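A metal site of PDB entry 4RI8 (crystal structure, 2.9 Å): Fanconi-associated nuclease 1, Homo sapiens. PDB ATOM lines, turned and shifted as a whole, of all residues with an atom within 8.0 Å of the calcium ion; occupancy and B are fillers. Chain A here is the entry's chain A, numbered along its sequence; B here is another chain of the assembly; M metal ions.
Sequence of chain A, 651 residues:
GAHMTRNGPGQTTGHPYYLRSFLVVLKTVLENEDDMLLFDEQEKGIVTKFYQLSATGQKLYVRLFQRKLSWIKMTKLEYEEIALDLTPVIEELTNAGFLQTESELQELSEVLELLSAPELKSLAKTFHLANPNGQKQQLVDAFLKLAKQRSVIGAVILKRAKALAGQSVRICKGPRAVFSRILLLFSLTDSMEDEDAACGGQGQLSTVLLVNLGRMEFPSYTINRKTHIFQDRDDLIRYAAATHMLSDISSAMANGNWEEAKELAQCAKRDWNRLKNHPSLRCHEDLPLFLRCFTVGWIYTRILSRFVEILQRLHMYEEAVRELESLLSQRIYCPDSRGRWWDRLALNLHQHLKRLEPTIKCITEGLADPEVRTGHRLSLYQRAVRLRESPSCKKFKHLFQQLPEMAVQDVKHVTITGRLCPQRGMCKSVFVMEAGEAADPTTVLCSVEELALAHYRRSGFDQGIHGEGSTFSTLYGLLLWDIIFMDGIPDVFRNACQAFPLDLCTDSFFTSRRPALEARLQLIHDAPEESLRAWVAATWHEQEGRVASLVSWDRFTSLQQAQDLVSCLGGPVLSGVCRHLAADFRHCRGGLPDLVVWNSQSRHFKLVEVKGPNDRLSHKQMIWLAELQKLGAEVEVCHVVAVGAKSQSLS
OP2 of DG 4 of chain B is in salt-bridge range of the side-chain amino group of Lys 611.
OE2 of Glu 609 lies close to NZ of Lys 611 (2.7 Å).
OE1 of Glu 609 lies within hydrogen-bond range of NE2 of Gln 621 (3.1 Å).
The backbone carbonyl oxygen of Asp 594 is in hydrogen-bond range of the backbone NH of Glu 468.
The side-chain amino group (NZ) of Lys 428 lies within salt-bridge range of the side-chain carboxylate (OE1) of Glu 449 (2.9 Å).
The side-chain carboxylate (OD2) of Asp 615 is in salt-bridge range of the side-chain amino group (NZ) of Lys 611 (3.0 Å).
The side-chain amino group (NZ) of Lys 611 sits close to the side-chain amide nitrogen (NE2) of Gln 621, at 3.2 Å.
The backbone NH (N) of Lys 611 is in hydrogen-bond range of the backbone carbonyl oxygen (O) of Cys 638 (2.9 Å).
Glu 449 touches the calcium ion.
NZ of Lys 611 touches the calcium ion (3.7 Å).
Of the 22 residues printed, 6 come within 4 Å of the calcium ion.
Along chain A the residues within 4 Å of the calcium ion span positions 449 to 611.
The calcium ion is bound by O of Val 610 (2.3 Å), OP1 of DG 4 of chain B (2.3 Å), OE2 of Glu 609 (2.3 Å) and OD2 of Asp 594 (2.3 Å).
Slightly farther from the calcium ion lies the side-chain carboxylate (OD1) of Asp 594 (3.0 Å).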
ATOM      1  N   LYS A 428     -15.491 -16.223   9.508  1.00  0.00           N
ATOM      2  CA  LYS A 428     -14.655 -17.385   9.201  1.00  0.00           C
ATOM      3  C   LYS A 428     -13.868 -17.205   7.892  1.00  0.00           C
ATOM      4  O   LYS A 428     -14.431 -16.787   6.874  1.00  0.00           O
ATOM      5  CB  LYS A 428     -15.479 -18.686   9.174  1.00  0.00           C
ATOM      6  CG  LYS A 428     -14.673 -19.912   9.589  1.00  0.00           C
ATOM      7  CD  LYS A 428     -15.172 -21.208   8.953  1.00  0.00           C
ATOM      8  CE  LYS A 428     -14.168 -22.354   9.172  1.00  0.00           C
ATOM      9  NZ  LYS A 428     -14.572 -23.674   8.622  1.00  0.00           N
ATOM     10  N   VAL A 448     -10.825 -22.981   5.182  1.00  0.00           N
ATOM     11  CA  VAL A 448      -9.442 -23.350   5.500  1.00  0.00           C
ATOM     12  C   VAL A 448      -9.263 -24.854   5.420  1.00  0.00           C
ATOM     13  O   VAL A 448      -8.356 -25.349   4.734  1.00  0.00           O
ATOM     14  CB  VAL A 448      -9.073 -22.928   6.935  1.00  0.00           C
ATOM     15  CG1 VAL A 448      -7.585 -23.110   7.203  1.00  0.00           C
ATOM     16  CG2 VAL A 448      -9.495 -21.487   7.171  1.00  0.00           C
ATOM     17  N   GLU A 449     -10.128 -25.569   6.131  1.00  0.00           N
ATOM     18  CA  GLU A 449     -10.076 -27.029   6.201  1.00  0.00           C
ATOM     19  C   GLU A 449     -10.319 -27.695   4.826  1.00  0.00           C
ATOM     20  O   GLU A 449      -9.693 -28.702   4.520  1.00  0.00           O
ATOM     21  CB  GLU A 449     -11.058 -27.560   7.263  1.00  0.00           C
ATOM     22  CG  GLU A 449     -10.655 -27.253   8.707  1.00  0.00           C
ATOM     23  CD  GLU A 449     -11.307 -25.990   9.291  1.00  0.00           C
ATOM     24  OE1 GLU A 449     -12.149 -25.354   8.595  1.00  0.00           O
ATOM     25  OE2 GLU A 449     -10.969 -25.640  10.461  1.00  0.00           O
ATOM     26  N   HIS A 466     -13.894 -33.826   6.702  1.00  0.00           N
ATOM     27  CA  HIS A 466     -13.814 -32.747   7.690  1.00  0.00           C
ATOM     28  C   HIS A 466     -14.911 -32.977   8.706  1.00  0.00           C
ATOM     29  O   HIS A 466     -16.021 -32.461   8.546  1.00  0.00           O
ATOM     30  CB  HIS A 466     -14.001 -31.390   7.025  1.00  0.00           C
ATOM     31  CG  HIS A 466     -14.012 -30.249   7.990  1.00  0.00           C
ATOM     32  ND1 HIS A 466     -13.432 -30.316   9.248  1.00  0.00           N
ATOM     33  CD2 HIS A 466     -14.526 -28.994   7.883  1.00  0.00           C
ATOM     34  CE1 HIS A 466     -13.592 -29.169   9.869  1.00  0.00           C
ATOM     35  NE2 HIS A 466     -14.263 -28.351   9.074  1.00  0.00           N
ATOM     36  N   GLU A 468     -14.136 -33.137  12.364  1.00  0.00           N
ATOM     37  CA  GLU A 468     -13.626 -32.882  13.720  1.00  0.00           C
ATOM     38  C   GLU A 468     -13.894 -34.112  14.583  1.00  0.00           C
ATOM     39  O   GLU A 468     -13.577 -35.247  14.202  1.00  0.00           O
ATOM     40  CB  GLU A 468     -14.226 -31.590  14.359  1.00  0.00           C
ATOM     41  CG  GLU A 468     -14.707 -30.500  13.392  1.00  0.00           C
ATOM     42  CD  GLU A 468     -14.171 -29.084  13.692  1.00  0.00           C
ATOM     43  OE1 GLU A 468     -14.214 -28.653  14.864  1.00  0.00           O
ATOM     44  OE2 GLU A 468     -13.698 -28.370  12.771  1.00  0.00           O
ATOM     45  N   LEU A 592     -10.433 -33.229  19.058  1.00  0.00           N
ATOM     46  CA  LEU A 592      -9.930 -34.166  18.058  1.00  0.00           C
ATOM     47  C   LEU A 592      -9.655 -33.400  16.764  1.00  0.00           C
ATOM     48  O   LEU A 592     -10.216 -32.328  16.577  1.00  0.00           O
ATOM     49  CB  LEU A 592     -10.909 -35.331  17.855  1.00  0.00           C
ATOM     50  CG  LEU A 592     -10.932 -36.348  19.019  1.00  0.00           C
ATOM     51  CD1 LEU A 592     -12.237 -37.116  19.013  1.00  0.00           C
ATOM     52  CD2 LEU A 592      -9.728 -37.284  18.938  1.00  0.00           C
ATOM     53  N   PRO A 593      -8.740 -33.907  15.909  1.00  0.00           N
ATOM     54  CA  PRO A 593      -8.348 -33.224  14.664  1.00  0.00           C
ATOM     55  C   PRO A 593      -9.481 -32.949  13.682  1.00  0.00           C
ATOM     56  O   PRO A 593     -10.364 -33.781  13.511  1.00  0.00           O
ATOM     57  CB  PRO A 593      -7.357 -34.193  14.030  1.00  0.00           C
ATOM     58  CG  PRO A 593      -6.972 -35.165  15.083  1.00  0.00           C
ATOM     59  CD  PRO A 593      -7.774 -34.923  16.311  1.00  0.00           C
ATOM     60  N   ASP A 594      -9.414 -31.797  13.023  1.00  0.00           N
ATOM     61  CA  ASP A 594     -10.472 -31.398  12.097  1.00  0.00           C
ATOM     62  C   ASP A 594     -10.763 -32.500  11.069  1.00  0.00           C
ATOM     63  O   ASP A 594     -11.930 -32.709  10.709  1.00  0.00           O
ATOM     64  CB  ASP A 594     -10.095 -30.110  11.357  1.00  0.00           C
ATOM     65  CG  ASP A 594      -9.957 -28.920  12.259  1.00  0.00           C
ATOM     66  OD1 ASP A 594     -10.967 -28.469  12.851  1.00  0.00           O
ATOM     67  OD2 ASP A 594      -8.816 -28.427  12.347  1.00  0.00           O
ATOM     68  N   LEU A 595      -9.701 -33.176  10.622  1.00  0.00           N
ATOM     69  CA  LEU A 595      -9.672 -33.993   9.412  1.00  0.00           C
ATOM     70  C   LEU A 595      -9.177 -35.442   9.613  1.00  0.00           C
ATOM     71  O   LEU A 595      -8.282 -35.680  10.438  1.00  0.00           O
ATOM     72  CB  LEU A 595      -8.741 -33.334   8.398  1.00  0.00           C
ATOM     73  CG  LEU A 595      -9.230 -32.427   7.259  1.00  0.00           C
ATOM     74  CD1 LEU A 595     -10.224 -31.384   7.708  1.00  0.00           C
ATOM     75  CD2 LEU A 595      -8.011 -31.780   6.622  1.00  0.00           C
ATOM     76  N   VAL A 608      -5.340 -35.014  10.825  1.00  0.00           N
ATOM     77  CA  VAL A 608      -4.793 -33.693  10.539  1.00  0.00           C
ATOM     78  C   VAL A 608      -5.584 -32.542  11.147  1.00  0.00           C
ATOM     79  O   VAL A 608      -6.749 -32.333  10.777  1.00  0.00           O
ATOM     80  CB  VAL A 608      -4.717 -33.487   9.014  1.00  0.00           C
ATOM     81  CG1 VAL A 608      -4.141 -32.122   8.684  1.00  0.00           C
ATOM     82  CG2 VAL A 608      -3.891 -34.594   8.375  1.00  0.00           C
ATOM     83  N   GLU A 609      -4.974 -31.798  12.070  1.00  0.00           N
ATOM     84  CA  GLU A 609      -5.558 -30.545  12.542  1.00  0.00           C
ATOM     85  C   GLU A 609      -5.155 -29.383  11.648  1.00  0.00           C
ATOM     86  O   GLU A 609      -3.969 -29.082  11.514  1.00  0.00           O
ATOM     87  CB  GLU A 609      -5.200 -30.243  13.999  1.00  0.00           C
ATOM     88  CG  GLU A 609      -5.607 -28.844  14.486  1.00  0.00           C
ATOM     89  CD  GLU A 609      -7.117 -28.562  14.558  1.00  0.00           C
ATOM     90  OE1 GLU A 609      -7.887 -29.417  15.049  1.00  0.00           O
ATOM     91  OE2 GLU A 609      -7.544 -27.462  14.147  1.00  0.00           O
ATOM     92  N   VAL A 610      -6.146 -28.737  11.057  1.00  0.00           N
ATOM     93  CA  VAL A 610      -5.932 -27.581  10.200  1.00  0.00           C
ATOM     94  C   VAL A 610      -5.992 -26.293  11.008  1.00  0.00           C
ATOM     95  O   VAL A 610      -6.990 -26.009  11.680  1.00  0.00           O
ATOM     96  CB  VAL A 610      -6.949 -27.530   9.047  1.00  0.00           C
ATOM     97  CG1 VAL A 610      -6.634 -26.377   8.093  1.00  0.00           C
ATOM     98  CG2 VAL A 610      -6.938 -28.846   8.293  1.00  0.00           C
ATOM     99  N   LYS A 611      -4.915 -25.525  10.929  1.00  0.00           N
ATOM    100  CA  LYS A 611      -4.743 -24.298  11.683  1.00  0.00           C
ATOM    101  C   LYS A 611      -4.536 -23.169  10.702  1.00  0.00           C
ATOM    102  O   LYS A 611      -3.587 -23.181   9.935  1.00  0.00           O
ATOM    103  CB  LYS A 611      -3.506 -24.417  12.583  1.00  0.00           C
ATOM    104  CG  LYS A 611      -3.691 -25.325  13.778  1.00  0.00           C
ATOM    105  CD  LYS A 611      -4.534 -24.627  14.805  1.00  0.00           C
ATOM    106  CE  LYS A 611      -5.179 -25.597  15.765  1.00  0.00           C
ATOM    107  NZ  LYS A 611      -6.652 -25.379  15.673  1.00  0.00           N
ATOM    108  N   GLY A 612      -5.448 -22.191  10.713  1.00  0.00           N
ATOM    109  CA  GLY A 612      -5.349 -21.049   9.802  1.00  0.00           C
ATOM    110  C   GLY A 612      -4.193 -20.142  10.181  1.00  0.00           C
ATOM    111  O   GLY A 612      -3.469 -20.434  11.142  1.00  0.00           O
ATOM    112  N   ASP A 615      -4.562 -18.962  14.093  1.00  0.00           N
ATOM    113  CA  ASP A 615      -4.653 -19.833  15.283  1.00  0.00           C
ATOM    114  C   ASP A 615      -3.570 -20.891  15.475  1.00  0.00           C
ATOM    115  O   ASP A 615      -2.916 -21.340  14.538  1.00  0.00           O
ATOM    116  CB  ASP A 615      -6.072 -20.420  15.477  1.00  0.00           C
ATOM    117  CG  ASP A 615      -6.489 -21.361  14.346  1.00  0.00           C
ATOM    118  OD1 ASP A 615      -6.498 -20.929  13.174  1.00  0.00           O
ATOM    119  OD2 ASP A 615      -6.855 -22.527  14.645  1.00  0.00           O
ATOM    120  N   ARG A 616      -3.386 -21.249  16.746  1.00  0.00           N
ATOM    121  CA  ARG A 616      -2.492 -22.309  17.181  1.00  0.00           C
ATOM    122  C   ARG A 616      -3.346 -23.370  17.932  1.00  0.00           C
ATOM    123  O   ARG A 616      -4.584 -23.275  17.986  1.00  0.00           O
ATOM    124  CB  ARG A 616      -1.379 -21.741  18.068  1.00  0.00           C
ATOM    125  CG  ARG A 616      -0.632 -20.549  17.472  1.00  0.00           C
ATOM    126  CD  ARG A 616       0.724 -20.262  18.130  1.00  0.00           C
ATOM    127  NE  ARG A 616       0.671 -19.231  19.173  1.00  0.00           N
ATOM    128  CZ  ARG A 616       0.459 -19.446  20.473  1.00  0.00           C
ATOM    129  NH1 ARG A 616       0.268 -20.681  20.928  1.00  0.00           N
ATOM    130  NH2 ARG A 616       0.449 -18.417  21.329  1.00  0.00           N
ATOM    131  N   LEU A 617      -2.665 -24.369  18.514  1.00  0.00           N
ATOM    132  CA  LEU A 617      -3.303 -25.528  19.122  1.00  0.00           C
ATOM    133  C   LEU A 617      -3.845 -25.211  20.478  1.00  0.00           C
ATOM    134  O   LEU A 617      -3.116 -24.673  21.300  1.00  0.00           O
ATOM    135  CB  LEU A 617      -2.284 -26.644  19.311  1.00  0.00           C
ATOM    136  CG  LEU A 617      -1.669 -27.357  18.095  1.00  0.00           C
ATOM    137  CD1 LEU A 617      -0.608 -28.325  18.587  1.00  0.00           C
ATOM    138  CD2 LEU A 617      -2.724 -28.082  17.250  1.00  0.00           C
ATOM    139  N   GLN A 621      -6.475 -30.061  22.075  1.00  0.00           N
ATOM    140  CA  GLN A 621      -5.922 -30.473  20.803  1.00  0.00           C
ATOM    141  C   GLN A 621      -4.585 -31.162  20.929  1.00  0.00           C
ATOM    142  O   GLN A 621      -4.381 -32.212  20.324  1.00  0.00           O
ATOM    143  CB  GLN A 621      -5.782 -29.289  19.874  1.00  0.00           C
ATOM    144  CG  GLN A 621      -7.005 -29.132  19.016  1.00  0.00           C
ATOM    145  CD  GLN A 621      -7.199 -27.731  18.508  1.00  0.00           C
ATOM    146  OE1 GLN A 621      -6.577 -26.785  18.969  1.00  0.00           O
ATOM    147  NE2 GLN A 621      -8.073 -27.587  17.548  1.00  0.00           N
ATOM    148  N   CYS A 638      -1.475 -28.956  10.089  1.00  0.00           N
ATOM    149  CA  CYS A 638      -1.338 -28.346   8.792  1.00  0.00           C
ATOM    150  C   CYS A 638      -1.665 -26.866   8.936  1.00  0.00           C
ATOM    151  O   CYS A 638      -2.795 -26.482   9.252  1.00  0.00           O
ATOM    152  CB  CYS A 638      -2.277 -29.035   7.805  1.00  0.00           C
ATOM    153  SG  CYS A 638      -2.361 -28.303   6.157  1.00  0.00           S
ATOM    154  P    DG B   3     -13.419 -28.542  20.309  1.00  0.00           P
ATOM    155  OP1  DG B   3     -13.426 -29.985  19.920  1.00  0.00           O
ATOM    156  OP2  DG B   3     -12.533 -28.059  21.398  1.00  0.00           O
ATOM    157  O5'  DG B   3     -13.095 -27.705  18.987  1.00  0.00           O
ATOM    158  C5'  DG B   3     -14.151 -27.192  18.137  1.00  0.00           C
ATOM    159  C4'  DG B   3     -13.872 -25.755  17.744  1.00  0.00           C
ATOM    160  O4'  DG B   3     -14.520 -24.846  18.656  1.00  0.00           O
ATOM    161  C3'  DG B   3     -12.396 -25.349  17.734  1.00  0.00           C
ATOM    162  O3'  DG B   3     -11.960 -25.412  16.365  1.00  0.00           O
ATOM    163  C2'  DG B   3     -12.386 -23.956  18.364  1.00  0.00           C
ATOM    164  C1'  DG B   3     -13.860 -23.605  18.515  1.00  0.00           C
ATOM    165  N9   DG B   3     -14.210 -22.761  19.663  1.00  0.00           N
ATOM    166  C8   DG B   3     -13.787 -22.888  20.963  1.00  0.00           C
ATOM    167  N7   DG B   3     -14.270 -21.967  21.754  1.00  0.00           N
ATOM    168  C5   DG B   3     -15.056 -21.172  20.920  1.00  0.00           C
ATOM    169  C6   DG B   3     -15.828 -20.017  21.212  1.00  0.00           C
ATOM    170  O6   DG B   3     -15.986 -19.442  22.290  1.00  0.00           O
ATOM    171  N1   DG B   3     -16.473 -19.532  20.071  1.00  0.00           N
ATOM    172  C2   DG B   3     -16.376 -20.089  18.818  1.00  0.00           C
ATOM    173  N2   DG B   3     -17.068 -19.482  17.850  1.00  0.00           N
ATOM    174  N3   DG B   3     -15.659 -21.159  18.536  1.00  0.00           N
ATOM    175  C4   DG B   3     -15.029 -21.649  19.620  1.00  0.00           C
ATOM    176  P    DG B   4     -10.600 -24.719  15.874  1.00  0.00           P
ATOM    177  OP1  DG B   4      -9.981 -25.614  14.852  1.00  0.00           O
ATOM    178  OP2  DG B   4      -9.821 -24.312  17.067  1.00  0.00           O
ATOM    179  O5'  DG B   4     -11.129 -23.425  15.122  1.00  0.00           O
ATOM    180  C5'  DG B   4     -12.231 -23.525  14.207  1.00  0.00           C
ATOM    181  C4'  DG B   4     -12.598 -22.156  13.672  1.00  0.00           C
ATOM    182  O4'  DG B   4     -13.236 -21.377  14.713  1.00  0.00           O
ATOM    183  C3'  DG B   4     -11.425 -21.328  13.162  1.00  0.00           C
ATOM    184  O3'  DG B   4     -11.799 -20.737  11.910  1.00  0.00           O
ATOM    185  C2'  DG B   4     -11.188 -20.295  14.260  1.00  0.00           C
ATOM    186  C1'  DG B   4     -12.567 -20.142  14.907  1.00  0.00           C
ATOM    187  N9   DG B   4     -12.536 -19.881  16.349  1.00  0.00           N
ATOM    188  C8   DG B   4     -11.826 -20.589  17.296  1.00  0.00           C
ATOM    189  N7   DG B   4     -12.006 -20.136  18.505  1.00  0.00           N
ATOM    190  C5   DG B   4     -12.892 -19.084  18.349  1.00  0.00           C
ATOM    191  C6   DG B   4     -13.463 -18.206  19.324  1.00  0.00           C
ATOM    192  O6   DG B   4     -13.282 -18.190  20.545  1.00  0.00           O
ATOM    193  N1   DG B   4     -14.308 -17.277  18.732  1.00  0.00           N
ATOM    194  C2   DG B   4     -14.578 -17.196  17.385  1.00  0.00           C
ATOM    195  N2   DG B   4     -15.430 -16.230  17.019  1.00  0.00           N
ATOM    196  N3   DG B   4     -14.059 -18.000  16.480  1.00  0.00           N
ATOM    197  C4   DG B   4     -13.236 -18.915  17.029  1.00  0.00           C
ATOM    198  P    DC B   5     -10.688 -20.189  10.904  1.00  0.00           P
ATOM    199  OP1  DC B   5     -11.154 -20.430   9.519  1.00  0.00           O
ATOM    200  OP2  DC B   5      -9.361 -20.711  11.336  1.00  0.00           O
ATOM    201  O5'  DC B   5     -10.787 -18.611  11.138  1.00  0.00           O
ATOM    202  C5'  DC B   5     -12.079 -17.978  11.231  1.00  0.00           C
ATOM    203  C4'  DC B   5     -11.961 -16.573  11.792  1.00  0.00           C
ATOM    204  O4'  DC B   5     -12.176 -16.607  13.229  1.00  0.00           O
ATOM    205  C3'  DC B   5     -10.609 -15.903  11.573  1.00  0.00           C
ATOM    206  O3'  DC B   5     -10.762 -14.573  11.080  1.00  0.00           O
ATOM    207  C2'  DC B   5     -10.010 -15.839  12.970  1.00  0.00           C
ATOM    208  C1'  DC B   5     -11.249 -15.733  13.822  1.00  0.00           C
ATOM    209  N1   DC B   5     -11.055 -16.124  15.228  1.00  0.00           N
ATOM    210  C2   DC B   5     -11.801 -15.485  16.213  1.00  0.00           C
ATOM    211  O2   DC B   5     -12.660 -14.651  15.875  1.00  0.00           O
ATOM    212  N3   DC B   5     -11.578 -15.788  17.515  1.00  0.00           N
ATOM    213  C4   DC B   5     -10.647 -16.682  17.838  1.00  0.00           C
ATOM    214  N4   DC B   5     -10.468 -16.960  19.131  1.00  0.00           N
ATOM    215  C5   DC B   5      -9.851 -17.341  16.851  1.00  0.00           C
ATOM    216  C6   DC B   5     -10.080 -17.027  15.576  1.00  0.00           C
HETATM  217 CA    CA M   1      -8.962 -26.173  12.854  1.00  0.00          CA
